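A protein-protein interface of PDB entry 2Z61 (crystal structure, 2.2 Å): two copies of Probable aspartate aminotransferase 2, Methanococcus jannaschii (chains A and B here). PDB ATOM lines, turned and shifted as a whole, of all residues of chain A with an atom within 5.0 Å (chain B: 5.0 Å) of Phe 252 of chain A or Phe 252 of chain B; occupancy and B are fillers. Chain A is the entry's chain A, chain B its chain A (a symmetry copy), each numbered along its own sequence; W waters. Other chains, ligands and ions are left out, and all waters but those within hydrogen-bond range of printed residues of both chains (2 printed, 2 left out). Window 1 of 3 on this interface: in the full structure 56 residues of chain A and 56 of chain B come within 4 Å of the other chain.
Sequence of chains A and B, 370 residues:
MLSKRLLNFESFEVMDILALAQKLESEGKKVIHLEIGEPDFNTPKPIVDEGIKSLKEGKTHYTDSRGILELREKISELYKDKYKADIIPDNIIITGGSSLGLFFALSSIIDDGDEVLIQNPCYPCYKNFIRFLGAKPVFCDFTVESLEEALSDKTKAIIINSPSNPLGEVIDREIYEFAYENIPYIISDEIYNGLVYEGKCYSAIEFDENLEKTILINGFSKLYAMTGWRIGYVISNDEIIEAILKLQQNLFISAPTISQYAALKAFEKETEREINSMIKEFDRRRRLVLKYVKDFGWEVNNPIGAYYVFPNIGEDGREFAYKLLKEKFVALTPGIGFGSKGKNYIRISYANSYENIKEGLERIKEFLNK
The backbone NH (N) of Leu 100 of chain B lies within hydrogen-bond range of the backbone carbonyl oxygen (O) of Leu 251 of chain A (3.4 Å).
The backbone carbonyl oxygen (O) of Phe 252 of chain B lies within hydrogen-bond range of the guanidinium group (NH1) of Arg 230 of chain A (2.9 Å).
The backbone NH of Leu 100 of chain A lies within hydrogen-bond range of the backbone carbonyl oxygen of Leu 251 of chain B (3.4 Å).
The backbone carbonyl oxygen of Phe 252 of chain A sits at hydrogen-bond distance from the guanidinium group of Arg 230 of chain B, at 2.9 Å.
Among the printed residues, merely in contact across the chains: Gly 96 of chain A with Phe 252 of chain B (3.1 Å), Ser 99 of chain A with Asn 250 of chain B (3.8 Å), Ser 99 of chain A with Leu 251 of chain B (3.2 Å), Arg 230 of chain A with Ser 254 of chain B (2.9 Å), Arg 230 of chain A with Pro 256 of chain B (3.7 Å), Asn 250 of chain A with Ser 99 of chain B (3.8 Å), Leu 251 of chain A with Ser 99 of chain B (3.2 Å), Phe 252 of chain A with Gly 96 of chain B (3.1 Å), Phe 252 of chain A with Phe 252 of chain B (3.8 Å), Ser 254 of chain A with Arg 230 of chain B (2.9 Å) and Pro 256 of chain A with Arg 230 of chain B (3.7 Å).
Of the printed residues of chain B, Ser 99 of chain A touches Asn 250 and Leu 251.
Of the printed residues of chain B, Leu 100 of chain A touches Leu 251.
Of the printed residues of chain B, Leu 251 of chain A touches Ser 99 (3.2 Å) and Leu 100 (3.4 Å).
Of chain B, only Gly 96 (3.1 Å), Arg 230 (2.9 Å) and Phe 252 (3.8 Å) come within 4 Å of Phe 252 of chain A.
Ile 253 of chain A touches none of the printed residues of chain B.
Of the printed residues of chain A, Gly 96 of chain B touches Phe 252 (3.1 Å).
Of the printed residues of chain A, Pro 256 of chain B touches Arg 230.
The nearest residue of chain B that does not touch Phe 252 of chain A is Leu 100 of chain B (4.1 Å).
The nearest residue of chain A that does not touch Phe 252 of chain B is Leu 100 of chain A (4.1 Å).
The nearest printed residue of chain A that does not touch Ser 99 of chain B is Ile 253 of chain A (4.1 Å).
Printed residues of chain B that touch a printed residue of chain A: Gly 96, Ser 99, Leu 100, Arg 230, Asn 250, Leu 251, Phe 252, Ser 254 and Pro 256.
Of the 16 printed residues of chain A, 9 touch a printed residue of chain B.
Hydrophobic or aromatic side chains of chain A within 4 Å of the printed part of chain B: Leu 100, Phe 252 and Pro 256.
Among the printed residues, 15 pairs touch across the chains.
Among the printed residues, no Asp or Glu carboxylate lies within 4 Å of a Lys or Arg side-chain nitrogen of the other chain.
Gly 96 of chain A touches Phe 252 of chain B, and with the chains exchanged Phe 252 of chain A touches Gly 96 of chain B.
Leu 100 of chain A touches Leu 251 of chain B, and with the chains exchanged Leu 251 of chain A touches Leu 100 of chain B.
Arg 230 of chain A touches Phe 252 of chain B, and with the chains exchanged Phe 252 of chain A touches Arg 230 of chain B.
Arg 230 of chain A touches Pro 256 of chain B, and with the chains exchanged Pro 256 of chain A touches Arg 230 of chain B.
Positions printed for both chains: 95, 96, 99, 100, 104, 230, 247, 248, 249, 250, 251, 252, 253, 254, 255 and 256.
Of the 15 pairs that touch across the chains among the printed residues, 15 have their exchanged pair printed and touching as well.
Water W2 lies within hydrogen-bond range of the backbone carbonyl oxygen (O) of Asn 250 of chain B (2.8 Å) and the side-chain hydroxyl (OG) of Ser 99 of chain A (2.8 Å).
Water W1 bridges O of Asn 250 of chain A (2.8 Å) and OG of Ser 99 of chain B (2.8 Å).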
ATOM      1  N   THR A  95      -9.012 -25.527 -13.364  1.00  0.00           N
ATOM      2  CA  THR A  95      -9.546 -24.957 -14.606  1.00  0.00           C
ATOM      3  C   THR A  95      -8.617 -25.211 -15.791  1.00  0.00           C
ATOM      4  O   THR A  95      -7.490 -25.679 -15.625  1.00  0.00           O
ATOM      5  CB  THR A  95      -9.742 -23.423 -14.478  1.00  0.00           C
ATOM      6  OG1 THR A  95      -8.505 -22.813 -14.079  1.00  0.00           O
ATOM      7  CG2 THR A  95     -10.794 -23.098 -13.442  1.00  0.00           C
ATOM      8  N   GLY A  96      -9.092 -24.884 -16.987  1.00  0.00           N
ATOM      9  CA  GLY A  96      -8.276 -25.065 -18.176  1.00  0.00           C
ATOM     10  C   GLY A  96      -7.447 -23.818 -18.385  1.00  0.00           C
ATOM     11  O   GLY A  96      -7.636 -23.089 -19.354  1.00  0.00           O
ATOM     12  N   SER A  99      -6.618 -18.047 -17.455  1.00  0.00           N
ATOM     13  CA  SER A  99      -7.517 -17.147 -18.171  1.00  0.00           C
ATOM     14  C   SER A  99      -8.982 -17.544 -17.989  1.00  0.00           C
ATOM     15  O   SER A  99      -9.823 -16.692 -17.711  1.00  0.00           O
ATOM     16  CB  SER A  99      -7.166 -17.124 -19.660  1.00  0.00           C
ATOM     17  OG  SER A  99      -5.897 -16.523 -19.853  1.00  0.00           O
ATOM     18  N   LEU A 100      -9.290 -18.832 -18.154  1.00  0.00           N
ATOM     19  CA  LEU A 100     -10.662 -19.282 -17.967  1.00  0.00           C
ATOM     20  C   LEU A 100     -11.070 -19.103 -16.514  1.00  0.00           C
ATOM     21  O   LEU A 100     -12.199 -18.730 -16.231  1.00  0.00           O
ATOM     22  CB  LEU A 100     -10.834 -20.759 -18.352  1.00  0.00           C
ATOM     23  CG  LEU A 100     -11.494 -21.044 -19.704  1.00  0.00           C
ATOM     24  CD1 LEU A 100     -11.878 -22.522 -19.778  1.00  0.00           C
ATOM     25  CD2 LEU A 100     -12.736 -20.165 -19.866  1.00  0.00           C
ATOM     26  N   PHE A 104     -14.387 -17.104 -15.305  1.00  0.00           N
ATOM     27  CA  PHE A 104     -15.427 -17.735 -14.505  1.00  0.00           C
ATOM     28  C   PHE A 104     -15.657 -16.980 -13.195  1.00  0.00           C
ATOM     29  O   PHE A 104     -16.791 -16.874 -12.722  1.00  0.00           O
ATOM     30  CB  PHE A 104     -15.047 -19.188 -14.199  1.00  0.00           C
ATOM     31  CG  PHE A 104     -15.111 -20.111 -15.389  1.00  0.00           C
ATOM     32  CD1 PHE A 104     -14.611 -21.410 -15.301  1.00  0.00           C
ATOM     33  CD2 PHE A 104     -15.694 -19.699 -16.584  1.00  0.00           C
ATOM     34  CE1 PHE A 104     -14.692 -22.290 -16.388  1.00  0.00           C
ATOM     35  CE2 PHE A 104     -15.780 -20.569 -17.673  1.00  0.00           C
ATOM     36  CZ  PHE A 104     -15.277 -21.868 -17.574  1.00  0.00           C
ATOM     37  N   ARG A 230      -2.268 -25.925 -20.341  1.00  0.00           N
ATOM     38  CA  ARG A 230      -3.567 -25.337 -19.995  1.00  0.00           C
ATOM     39  C   ARG A 230      -4.165 -25.857 -18.693  1.00  0.00           C
ATOM     40  O   ARG A 230      -5.120 -26.643 -18.693  1.00  0.00           O
ATOM     41  CB  ARG A 230      -4.581 -25.574 -21.127  1.00  0.00           C
ATOM     42  CG  ARG A 230      -4.096 -25.234 -22.529  1.00  0.00           C
ATOM     43  CD  ARG A 230      -4.127 -23.748 -22.765  1.00  0.00           C
ATOM     44  NE  ARG A 230      -3.094 -23.116 -21.980  1.00  0.00           N
ATOM     45  CZ  ARG A 230      -3.240 -21.984 -21.315  1.00  0.00           C
ATOM     46  NH1 ARG A 230      -4.393 -21.325 -21.336  1.00  0.00           N
ATOM     47  NH2 ARG A 230      -2.224 -21.544 -20.602  1.00  0.00           N
ATOM     48  N   LEU A 247     -20.475 -23.279 -14.098  1.00  0.00           N
ATOM     49  CA  LEU A 247     -19.940 -22.693 -15.319  1.00  0.00           C
ATOM     50  C   LEU A 247     -18.971 -23.677 -15.975  1.00  0.00           C
ATOM     51  O   LEU A 247     -18.999 -23.881 -17.192  1.00  0.00           O
ATOM     52  CB  LEU A 247     -19.210 -21.384 -15.008  1.00  0.00           C
ATOM     53  CG  LEU A 247     -20.078 -20.193 -14.599  1.00  0.00           C
ATOM     54  CD1 LEU A 247     -19.195 -19.077 -14.090  1.00  0.00           C
ATOM     55  CD2 LEU A 247     -20.907 -19.719 -15.790  1.00  0.00           C
ATOM     56  N   GLN A 248     -18.116 -24.287 -15.158  1.00  0.00           N
ATOM     57  CA  GLN A 248     -17.132 -25.252 -15.640  1.00  0.00           C
ATOM     58  C   GLN A 248     -17.780 -26.498 -16.247  1.00  0.00           C
ATOM     59  O   GLN A 248     -17.345 -26.976 -17.293  1.00  0.00           O
ATOM     60  CB  GLN A 248     -16.192 -25.663 -14.501  1.00  0.00           C
ATOM     61  CG  GLN A 248     -15.278 -26.844 -14.837  1.00  0.00           C
ATOM     62  CD  GLN A 248     -13.814 -26.446 -14.944  1.00  0.00           C
ATOM     63  OE1 GLN A 248     -13.465 -25.505 -15.644  1.00  0.00           O
ATOM     64  NE2 GLN A 248     -12.953 -27.172 -14.247  1.00  0.00           N
ATOM     65  N   GLN A 249     -18.816 -27.019 -15.598  1.00  0.00           N
ATOM     66  CA  GLN A 249     -19.502 -28.210 -16.093  1.00  0.00           C
ATOM     67  C   GLN A 249     -20.158 -27.983 -17.452  1.00  0.00           C
ATOM     68  O   GLN A 249     -20.275 -28.909 -18.256  1.00  0.00           O
ATOM     69  CB  GLN A 249     -20.571 -28.670 -15.100  1.00  0.00           C
ATOM     70  CG  GLN A 249     -20.045 -29.010 -13.727  1.00  0.00           C
ATOM     71  CD  GLN A 249     -21.160 -29.281 -12.736  1.00  0.00           C
ATOM     72  OE1 GLN A 249     -21.993 -28.414 -12.477  1.00  0.00           O
ATOM     73  NE2 GLN A 249     -21.178 -30.485 -12.175  1.00  0.00           N
ATOM     74  N   ASN A 250     -20.583 -26.753 -17.710  1.00  0.00           N
ATOM     75  CA  ASN A 250     -21.235 -26.437 -18.974  1.00  0.00           C
ATOM     76  C   ASN A 250     -20.272 -26.045 -20.091  1.00  0.00           C
ATOM     77  O   ASN A 250     -20.315 -26.618 -21.182  1.00  0.00           O
ATOM     78  CB  ASN A 250     -22.262 -25.310 -18.773  1.00  0.00           C
ATOM     79  CG  ASN A 250     -23.568 -25.805 -18.157  1.00  0.00           C
ATOM     80  OD1 ASN A 250     -24.514 -26.149 -18.871  1.00  0.00           O
ATOM     81  ND2 ASN A 250     -23.620 -25.849 -16.830  1.00  0.00           N
ATOM     82  N   LEU A 251     -19.395 -25.086 -19.803  1.00  0.00           N
ATOM     83  CA  LEU A 251     -18.457 -24.554 -20.786  1.00  0.00           C
ATOM     84  C   LEU A 251     -17.163 -25.301 -21.088  1.00  0.00           C
ATOM     85  O   LEU A 251     -16.605 -25.140 -22.176  1.00  0.00           O
ATOM     86  CB  LEU A 251     -18.080 -23.116 -20.406  1.00  0.00           C
ATOM     87  CG  LEU A 251     -19.152 -22.022 -20.389  1.00  0.00           C
ATOM     88  CD1 LEU A 251     -19.765 -21.920 -21.759  1.00  0.00           C
ATOM     89  CD2 LEU A 251     -20.223 -22.322 -19.355  1.00  0.00           C
ATOM     90  N   PHE A 252     -16.674 -26.114 -20.157  1.00  0.00           N
ATOM     91  CA  PHE A 252     -15.398 -26.782 -20.385  1.00  0.00           C
ATOM     92  C   PHE A 252     -15.339 -28.263 -19.992  1.00  0.00           C
ATOM     93  O   PHE A 252     -14.553 -29.029 -20.555  1.00  0.00           O
ATOM     94  CB  PHE A 252     -14.313 -25.996 -19.634  1.00  0.00           C
ATOM     95  CG  PHE A 252     -12.925 -26.260 -20.121  1.00  0.00           C
ATOM     96  CD1 PHE A 252     -12.573 -25.977 -21.434  1.00  0.00           C
ATOM     97  CD2 PHE A 252     -11.977 -26.815 -19.277  1.00  0.00           C
ATOM     98  CE1 PHE A 252     -11.296 -26.251 -21.899  1.00  0.00           C
ATOM     99  CE2 PHE A 252     -10.690 -27.094 -19.735  1.00  0.00           C
ATOM    100  CZ  PHE A 252     -10.351 -26.814 -21.046  1.00  0.00           C
ATOM    101  N   ILE A 253     -16.172 -28.654 -19.031  1.00  0.00           N
ATOM    102  CA  ILE A 253     -16.231 -30.025 -18.520  1.00  0.00           C
ATOM    103  C   ILE A 253     -15.125 -30.279 -17.486  1.00  0.00           C
ATOM    104  O   ILE A 253     -15.418 -30.520 -16.320  1.00  0.00           O
ATOM    105  CB  ILE A 253     -16.116 -31.079 -19.643  1.00  0.00           C
ATOM    106  CG1 ILE A 253     -17.107 -30.771 -20.776  1.00  0.00           C
ATOM    107  CG2 ILE A 253     -16.393 -32.463 -19.068  1.00  0.00           C
ATOM    108  CD1 ILE A 253     -18.558 -30.850 -20.379  1.00  0.00           C
ATOM    109  N   SER A 254     -13.858 -30.230 -17.903  1.00  0.00           N
ATOM    110  CA  SER A 254     -12.743 -30.445 -16.971  1.00  0.00           C
ATOM    111  C   SER A 254     -11.384 -30.171 -17.616  1.00  0.00           C
ATOM    112  O   SER A 254     -11.225 -30.319 -18.826  1.00  0.00           O
ATOM    113  CB  SER A 254     -12.773 -31.876 -16.411  1.00  0.00           C
ATOM    114  OG  SER A 254     -12.612 -32.863 -17.422  1.00  0.00           O
ATOM    115  N   ALA A 255     -10.407 -29.757 -16.811  1.00  0.00           N
ATOM    116  CA  ALA A 255      -9.074 -29.458 -17.315  1.00  0.00           C
ATOM    117  C   ALA A 255      -8.486 -30.695 -17.989  1.00  0.00           C
ATOM    118  O   ALA A 255      -8.836 -31.824 -17.649  1.00  0.00           O
ATOM    119  CB  ALA A 255      -8.163 -29.005 -16.177  1.00  0.00           C
ATOM    120  N   PRO A 256      -7.579 -30.500 -18.955  1.00  0.00           N
ATOM    121  CA  PRO A 256      -6.995 -31.663 -19.630  1.00  0.00           C
ATOM    122  C   PRO A 256      -6.464 -32.725 -18.659  1.00  0.00           C
ATOM    123  O   PRO A 256      -5.678 -32.448 -17.748  1.00  0.00           O
ATOM    124  CB  PRO A 256      -5.921 -31.050 -20.542  1.00  0.00           C
ATOM    125  CG  PRO A 256      -5.720 -29.659 -20.011  1.00  0.00           C
ATOM    126  CD  PRO A 256      -7.058 -29.240 -19.504  1.00  0.00           C
ATOM    127  N   THR B  95     -10.005 -25.174 -30.835  1.00  0.00           N
ATOM    128  CA  THR B  95     -10.469 -24.731 -29.515  1.00  0.00           C
ATOM    129  C   THR B  95     -10.144 -25.751 -28.428  1.00  0.00           C
ATOM    130  O   THR B  95      -9.710 -26.868 -28.715  1.00  0.00           O
ATOM    131  CB  THR B  95     -12.005 -24.506 -29.510  1.00  0.00           C
ATOM    132  OG1 THR B  95     -12.666 -25.701 -29.953  1.00  0.00           O
ATOM    133  CG2 THR B  95     -12.388 -23.373 -30.435  1.00  0.00           C
ATOM    134  N   GLY B  96     -10.369 -25.366 -27.177  1.00  0.00           N
ATOM    135  CA  GLY B  96     -10.114 -26.274 -26.071  1.00  0.00           C
ATOM    136  C   GLY B  96     -11.357 -27.101 -25.830  1.00  0.00           C
ATOM    137  O   GLY B  96     -12.006 -26.978 -24.796  1.00  0.00           O
ATOM    138  N   SER B  99     -17.195 -27.783 -26.373  1.00  0.00           N
ATOM    139  CA  SER B  99     -18.022 -26.931 -25.523  1.00  0.00           C
ATOM    140  C   SER B  99     -17.613 -25.462 -25.623  1.00  0.00           C
ATOM    141  O   SER B  99     -18.469 -24.591 -25.770  1.00  0.00           O
ATOM    142  CB  SER B  99     -17.938 -27.395 -24.067  1.00  0.00           C
ATOM    143  OG  SER B  99     -18.546 -28.668 -23.926  1.00  0.00           O
ATOM    144  N   LEU B 100     -16.311 -25.183 -25.536  1.00  0.00           N
ATOM    145  CA  LEU B 100     -15.851 -23.806 -25.651  1.00  0.00           C
ATOM    146  C   LEU B 100     -16.133 -23.286 -27.052  1.00  0.00           C
ATOM    147  O   LEU B 100     -16.506 -22.134 -27.218  1.00  0.00           O
ATOM    148  CB  LEU B 100     -14.346 -23.684 -25.369  1.00  0.00           C
ATOM    149  CG  LEU B 100     -13.948 -23.133 -23.998  1.00  0.00           C
ATOM    150  CD1 LEU B 100     -12.461 -22.775 -24.009  1.00  0.00           C
ATOM    151  CD2 LEU B 100     -14.789 -21.897 -23.674  1.00  0.00           C
ATOM    152  N   PHE B 104     -18.156 -19.860 -27.847  1.00  0.00           N
ATOM    153  CA  PHE B 104     -17.569 -18.769 -28.612  1.00  0.00           C
ATOM    154  C   PHE B 104     -18.418 -18.430 -29.839  1.00  0.00           C
ATOM    155  O   PHE B 104     -18.538 -17.261 -30.214  1.00  0.00           O
ATOM    156  CB  PHE B 104     -16.151 -19.143 -29.057  1.00  0.00           C
ATOM    157  CG  PHE B 104     -15.140 -19.182 -27.940  1.00  0.00           C
ATOM    158  CD1 PHE B 104     -13.860 -19.691 -28.166  1.00  0.00           C
ATOM    159  CD2 PHE B 104     -15.449 -18.689 -26.677  1.00  0.00           C
ATOM    160  CE1 PHE B 104     -12.899 -19.705 -27.147  1.00  0.00           C
ATOM    161  CE2 PHE B 104     -14.497 -18.698 -25.654  1.00  0.00           C
ATOM    162  CZ  PHE B 104     -13.218 -19.208 -25.892  1.00  0.00           C
ATOM    163  N   ARG B 230      -9.202 -32.440 -24.442  1.00  0.00           N
ATOM    164  CA  ARG B 230      -9.791 -31.112 -24.642  1.00  0.00           C
ATOM    165  C   ARG B 230      -9.360 -30.421 -25.931  1.00  0.00           C
ATOM    166  O   ARG B 230      -8.559 -29.479 -25.918  1.00  0.00           O
ATOM    167  CB  ARG B 230      -9.450 -30.191 -23.458  1.00  0.00           C
ATOM    168  CG  ARG B 230      -9.691 -30.779 -22.074  1.00  0.00           C
ATOM    169  CD  ARG B 230     -11.154 -30.748 -21.722  1.00  0.00           C
ATOM    170  NE  ARG B 230     -11.863 -31.708 -22.533  1.00  0.00           N
ATOM    171  CZ  ARG B 230     -13.040 -31.498 -23.095  1.00  0.00           C
ATOM    172  NH1 ARG B 230     -13.674 -30.342 -22.936  1.00  0.00           N
ATOM    173  NH2 ARG B 230     -13.551 -32.450 -23.847  1.00  0.00           N
ATOM    174  N   LEU B 247     -11.981 -13.775 -29.060  1.00  0.00           N
ATOM    175  CA  LEU B 247     -12.482 -14.395 -27.842  1.00  0.00           C
ATOM    176  C   LEU B 247     -11.469 -15.424 -27.340  1.00  0.00           C
ATOM    177  O   LEU B 247     -11.173 -15.493 -26.144  1.00  0.00           O
ATOM    178  CB  LEU B 247     -13.824 -15.083 -28.106  1.00  0.00           C
ATOM    179  CG  LEU B 247     -15.026 -14.171 -28.355  1.00  0.00           C
ATOM    180  CD1 LEU B 247     -16.194 -14.998 -28.842  1.00  0.00           C
ATOM    181  CD2 LEU B 247     -15.393 -13.431 -27.072  1.00  0.00           C
ATOM    182  N   GLN B 248     -10.938 -16.221 -28.264  1.00  0.00           N
ATOM    183  CA  GLN B 248      -9.958 -17.251 -27.934  1.00  0.00           C
ATOM    184  C   GLN B 248      -8.658 -16.667 -27.377  1.00  0.00           C
ATOM    185  O   GLN B 248      -8.110 -17.188 -26.408  1.00  0.00           O
ATOM    186  CB  GLN B 248      -9.652 -18.106 -29.170  1.00  0.00           C
ATOM    187  CG  GLN B 248      -8.466 -19.057 -28.996  1.00  0.00           C
ATOM    188  CD  GLN B 248      -8.881 -20.520 -28.971  1.00  0.00           C
ATOM    189  OE1 GLN B 248      -9.772 -20.910 -28.228  1.00  0.00           O
ATOM    190  NE2 GLN B 248      -8.226 -21.333 -29.784  1.00  0.00           N
ATOM    191  N   GLN B 249      -8.168 -15.591 -27.985  1.00  0.00           N
ATOM    192  CA  GLN B 249      -6.931 -14.960 -27.532  1.00  0.00           C
ATOM    193  C   GLN B 249      -7.042 -14.408 -26.114  1.00  0.00           C
ATOM    194  O   GLN B 249      -6.055 -14.365 -25.377  1.00  0.00           O
ATOM    195  CB  GLN B 249      -6.528 -13.823 -28.473  1.00  0.00           C
ATOM    196  CG  GLN B 249      -6.303 -14.246 -29.905  1.00  0.00           C
ATOM    197  CD  GLN B 249      -6.088 -13.062 -30.826  1.00  0.00           C
ATOM    198  OE1 GLN B 249      -6.956 -12.201 -30.953  1.00  0.00           O
ATOM    199  NE2 GLN B 249      -4.930 -13.016 -31.475  1.00  0.00           N
ATOM    200  N   ASN B 250      -8.241 -13.989 -25.730  1.00  0.00           N
ATOM    201  CA  ASN B 250      -8.448 -13.433 -24.399  1.00  0.00           C
ATOM    202  C   ASN B 250      -8.772 -14.474 -23.332  1.00  0.00           C
ATOM    203  O   ASN B 250      -8.116 -14.522 -22.288  1.00  0.00           O
ATOM    204  CB  ASN B 250      -9.568 -12.379 -24.434  1.00  0.00           C
ATOM    205  CG  ASN B 250      -9.098 -11.036 -24.985  1.00  0.00           C
ATOM    206  OD1 ASN B 250      -8.683 -10.153 -24.231  1.00  0.00           O
ATOM    207  ND2 ASN B 250      -9.153 -10.882 -26.305  1.00  0.00           N
ATOM    208  N   LEU B 251      -9.765 -15.314 -23.611  1.00  0.00           N
ATOM    209  CA  LEU B 251     -10.239 -16.318 -22.663  1.00  0.00           C
ATOM    210  C   LEU B 251      -9.495 -17.641 -22.520  1.00  0.00           C
ATOM    211  O   LEU B 251      -9.583 -18.280 -21.468  1.00  0.00           O
ATOM    212  CB  LEU B 251     -11.708 -16.647 -22.959  1.00  0.00           C
ATOM    213  CG  LEU B 251     -12.780 -15.564 -22.810  1.00  0.00           C
ATOM    214  CD1 LEU B 251     -12.766 -15.056 -21.394  1.00  0.00           C
ATOM    215  CD2 LEU B 251     -12.541 -14.420 -23.780  1.00  0.00           C
ATOM    216  N   PHE B 252      -8.764 -18.067 -23.545  1.00  0.00           N
ATOM    217  CA  PHE B 252      -8.104 -19.365 -23.466  1.00  0.00           C
ATOM    218  C   PHE B 252      -6.658 -19.411 -23.976  1.00  0.00           C
ATOM    219  O   PHE B 252      -5.866 -20.248 -23.535  1.00  0.00           O
ATOM    220  CB  PHE B 252      -8.964 -20.378 -24.235  1.00  0.00           C
ATOM    221  CG  PHE B 252      -8.690 -21.803 -23.877  1.00  0.00           C
ATOM    222  CD1 PHE B 252      -8.879 -22.252 -22.576  1.00  0.00           C
ATOM    223  CD2 PHE B 252      -8.218 -22.691 -24.830  1.00  0.00           C
ATOM    224  CE1 PHE B 252      -8.594 -23.564 -22.233  1.00  0.00           C
ATOM    225  CE2 PHE B 252      -7.929 -24.012 -24.494  1.00  0.00           C
ATOM    226  CZ  PHE B 252      -8.114 -24.447 -23.196  1.00  0.00           C
ATOM    227  N   ILE B 253      -6.326 -18.512 -24.898  1.00  0.00           N
ATOM    228  CA  ILE B 253      -4.998 -18.431 -25.508  1.00  0.00           C
ATOM    229  C   ILE B 253      -4.843 -19.457 -26.639  1.00  0.00           C
ATOM    230  O   ILE B 253      -4.686 -19.078 -27.795  1.00  0.00           O
ATOM    231  CB  ILE B 253      -3.863 -18.645 -24.481  1.00  0.00           C
ATOM    232  CG1 ILE B 253      -4.066 -17.741 -23.256  1.00  0.00           C
ATOM    233  CG2 ILE B 253      -2.523 -18.343 -25.138  1.00  0.00           C
ATOM    234  CD1 ILE B 253      -3.991 -16.265 -23.546  1.00  0.00           C
ATOM    235  N   SER B 254      -4.884 -20.751 -26.317  1.00  0.00           N
ATOM    236  CA  SER B 254      -4.760 -21.794 -27.345  1.00  0.00           C
ATOM    237  C   SER B 254      -5.010 -23.195 -26.785  1.00  0.00           C
ATOM    238  O   SER B 254      -4.773 -23.449 -25.606  1.00  0.00           O
ATOM    239  CB  SER B 254      -3.376 -21.739 -28.009  1.00  0.00           C
ATOM    240  OG  SER B 254      -2.318 -21.990 -27.093  1.00  0.00           O
ATOM    241  N   ALA B 255      -5.501 -24.102 -27.629  1.00  0.00           N
ATOM    242  CA  ALA B 255      -5.785 -25.466 -27.205  1.00  0.00           C
ATOM    243  C   ALA B 255      -4.511 -26.120 -26.675  1.00  0.00           C
ATOM    244  O   ALA B 255      -3.405 -25.759 -27.074  1.00  0.00           O
ATOM    245  CB  ALA B 255      -6.340 -26.281 -28.371  1.00  0.00           C
ATOM    246  N   PRO B 256      -4.649 -27.096 -25.769  1.00  0.00           N
ATOM    247  CA  PRO B 256      -3.449 -27.745 -25.232  1.00  0.00           C
ATOM    248  C   PRO B 256      -2.474 -28.213 -26.319  1.00  0.00           C
ATOM    249  O   PRO B 256      -2.834 -28.922 -27.264  1.00  0.00           O
ATOM    250  CB  PRO B 256      -4.011 -28.879 -24.360  1.00  0.00           C
ATOM    251  CG  PRO B 256      -5.441 -29.020 -24.795  1.00  0.00           C
ATOM    252  CD  PRO B 256      -5.873 -27.643 -25.165  1.00  0.00           C
HETATM  253  O   HOH W   1     -21.171 -28.731 -22.846  1.00  0.00           O
HETATM  254  O   HOH W   2      -5.868 -13.824 -20.732  1.00  0.00           O
